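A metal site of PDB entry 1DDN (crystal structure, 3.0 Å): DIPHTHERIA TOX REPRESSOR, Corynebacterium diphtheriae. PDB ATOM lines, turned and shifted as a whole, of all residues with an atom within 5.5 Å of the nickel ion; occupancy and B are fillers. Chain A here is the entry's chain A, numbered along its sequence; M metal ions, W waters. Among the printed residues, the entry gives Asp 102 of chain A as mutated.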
ATOM      1  N   LEU A   4      -9.140  -1.594 -23.014  1.00  0.00           N
ATOM      2  CA  LEU A   4      -8.174  -2.146 -23.930  1.00  0.00           C
ATOM      3  C   LEU A   4      -6.792  -1.552 -23.708  1.00  0.00           C
ATOM      4  O   LEU A   4      -5.863  -1.894 -24.412  1.00  0.00           O
ATOM      5  CB  LEU A   4      -8.650  -1.896 -25.370  1.00  0.00           C
ATOM      6  CG  LEU A   4      -9.677  -2.843 -26.025  1.00  0.00           C
ATOM      7  CD1 LEU A   4     -10.498  -3.539 -24.975  1.00  0.00           C
ATOM      8  CD2 LEU A   4     -10.601  -2.052 -26.957  1.00  0.00           C
ATOM      9  N   VAL A   5      -6.644  -0.693 -22.717  1.00  0.00           N
ATOM     10  CA  VAL A   5      -5.372  -0.029 -22.432  1.00  0.00           C
ATOM     11  C   VAL A   5      -4.945   0.770 -23.646  1.00  0.00           C
ATOM     12  O   VAL A   5      -4.470   1.894 -23.512  1.00  0.00           O
ATOM     13  CB  VAL A   5      -4.273  -1.036 -22.089  1.00  0.00           C
ATOM     14  CG1 VAL A   5      -2.950  -0.301 -21.879  1.00  0.00           C
ATOM     15  CG2 VAL A   5      -4.650  -1.807 -20.841  1.00  0.00           C
ATOM     16  N   MET A  10      -4.934  -3.330 -29.854  1.00  0.00           N
ATOM     17  CA  MET A  10      -5.802  -4.486 -29.717  1.00  0.00           C
ATOM     18  C   MET A  10      -6.572  -4.778 -31.032  1.00  0.00           C
ATOM     19  O   MET A  10      -7.121  -5.862 -31.217  1.00  0.00           O
ATOM     20  CB  MET A  10      -6.779  -4.287 -28.559  1.00  0.00           C
ATOM     21  CG  MET A  10      -6.100  -4.182 -27.201  1.00  0.00           C
ATOM     22  SD  MET A  10      -5.421  -5.750 -26.539  1.00  0.00           S
ATOM     23  CE  MET A  10      -6.652  -6.880 -27.169  1.00  0.00           C
ATOM     24  N   ARG A  13      -3.494  -6.354 -33.061  1.00  0.00           N
ATOM     25  CA  ARG A  13      -3.232  -7.696 -32.585  1.00  0.00           C
ATOM     26  C   ARG A  13      -4.341  -8.638 -33.001  1.00  0.00           C
ATOM     27  O   ARG A  13      -4.062  -9.701 -33.535  1.00  0.00           O
ATOM     28  CB  ARG A  13      -3.110  -7.745 -31.065  1.00  0.00           C
ATOM     29  CG  ARG A  13      -2.756  -9.134 -30.589  1.00  0.00           C
ATOM     30  CD  ARG A  13      -2.694  -9.201 -29.106  1.00  0.00           C
ATOM     31  NE  ARG A  13      -3.934  -9.735 -28.562  1.00  0.00           N
ATOM     32  CZ  ARG A  13      -4.080 -10.108 -27.301  1.00  0.00           C
ATOM     33  NH1 ARG A  13      -3.062  -9.994 -26.457  1.00  0.00           N
ATOM     34  NH2 ARG A  13      -5.250 -10.597 -26.871  1.00  0.00           N
ATOM     35  N   ALA A 101      -1.259 -10.161 -19.260  1.00  0.00           N
ATOM     36  CA  ALA A 101      -0.411  -9.841 -20.403  1.00  0.00           C
ATOM     37  C   ALA A 101      -1.220  -8.992 -21.372  1.00  0.00           C
ATOM     38  O   ALA A 101      -0.665  -8.164 -22.092  1.00  0.00           O
ATOM     39  CB  ALA A 101       0.060 -11.095 -21.084  1.00  0.00           C
ATOM     40  N   ASP A 102      -2.529  -9.181 -21.373  1.00  0.00           N
ATOM     41  CA  ASP A 102      -3.401  -8.414 -22.259  1.00  0.00           C
ATOM     42  C   ASP A 102      -3.260  -6.916 -21.973  1.00  0.00           C
ATOM     43  O   ASP A 102      -3.525  -6.100 -22.844  1.00  0.00           O
ATOM     44  CB  ASP A 102      -4.858  -8.846 -22.073  1.00  0.00           C
ATOM     45  CG  ASP A 102      -5.777  -8.349 -23.183  1.00  0.00           C
ATOM     46  OD1 ASP A 102      -5.342  -7.493 -23.992  1.00  0.00           O
ATOM     47  OD2 ASP A 102      -6.927  -8.825 -23.254  1.00  0.00           O
ATOM     48  N   ARG A 103      -2.825  -6.568 -20.771  1.00  0.00           N
ATOM     49  CA  ARG A 103      -2.648  -5.154 -20.392  1.00  0.00           C
ATOM     50  C   ARG A 103      -1.195  -4.732 -20.558  1.00  0.00           C
ATOM     51  O   ARG A 103      -0.901  -3.652 -21.075  1.00  0.00           O
ATOM     52  CB  ARG A 103      -3.068  -4.930 -18.945  1.00  0.00           C
ATOM     53  CG  ARG A 103      -4.548  -5.095 -18.731  1.00  0.00           C
ATOM     54  CD  ARG A 103      -5.054  -4.312 -17.540  1.00  0.00           C
ATOM     55  NE  ARG A 103      -5.433  -5.231 -16.480  1.00  0.00           N
ATOM     56  CZ  ARG A 103      -4.547  -5.963 -15.808  1.00  0.00           C
ATOM     57  NH1 ARG A 103      -3.272  -5.851 -16.115  1.00  0.00           N
ATOM     58  NH2 ARG A 103      -4.924  -6.801 -14.855  1.00  0.00           N
ATOM     59  N   GLU A 105       1.104  -5.885 -22.575  1.00  0.00           N
ATOM     60  CA  GLU A 105       1.543  -5.772 -23.975  1.00  0.00           C
ATOM     61  C   GLU A 105       1.591  -4.326 -24.477  1.00  0.00           C
ATOM     62  O   GLU A 105       2.349  -4.002 -25.393  1.00  0.00           O
ATOM     63  CB  GLU A 105       0.619  -6.592 -24.885  1.00  0.00           C
ATOM     64  CG  GLU A 105      -0.855  -6.493 -24.521  1.00  0.00           C
ATOM     65  CD  GLU A 105      -1.760  -7.284 -25.454  1.00  0.00           C
ATOM     66  OE1 GLU A 105      -1.237  -8.184 -26.148  1.00  0.00           O
ATOM     67  OE2 GLU A 105      -2.980  -7.012 -25.482  1.00  0.00           O
ATOM     68  N   HIS A 106       0.783  -3.467 -23.856  1.00  0.00           N
ATOM     69  CA  HIS A 106       0.704  -2.073 -24.259  1.00  0.00           C
ATOM     70  C   HIS A 106       1.561  -1.103 -23.471  1.00  0.00           C
ATOM     71  O   HIS A 106       1.426   0.101 -23.630  1.00  0.00           O
ATOM     72  CB  HIS A 106      -0.751  -1.616 -24.215  1.00  0.00           C
ATOM     73  CG  HIS A 106      -1.699  -2.641 -24.744  1.00  0.00           C
ATOM     74  ND1 HIS A 106      -1.736  -3.002 -26.070  1.00  0.00           N
ATOM     75  CD2 HIS A 106      -2.564  -3.462 -24.105  1.00  0.00           C
ATOM     76  CE1 HIS A 106      -2.585  -4.008 -26.226  1.00  0.00           C
ATOM     77  NE2 HIS A 106      -3.093  -4.313 -25.046  1.00  0.00           N
HETATM   78 NI    NI M   1      -4.337  -5.840 -24.593  1.00  0.00          NI
HETATM   79  O   HOH W   1      -5.656  -4.565 -23.669  1.00  0.00           O
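The guanidinium group (NH1) of Arg 13 lies within salt-bridge range of the side-chain carboxylate (OE1) of Glu 105 (2.6 Å).
Within 4 Å of the nickel ion: Met 10, Asp 102, Glu 105 and His 106.
The nickel ion is bound by O of Asp 102 (1.9 Å). OE2 of Glu 105 binds the nickel ion (2.0 Å). The nickel ion is bound by NE2 of His 106 (2.0 Å). OD1 of Asp 102 is bound to the nickel ion (2.0 Å). Water W1 binds the nickel ion, at 2.1 Å. SD of Met 10 binds the nickel ion, 2.2 Å away.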
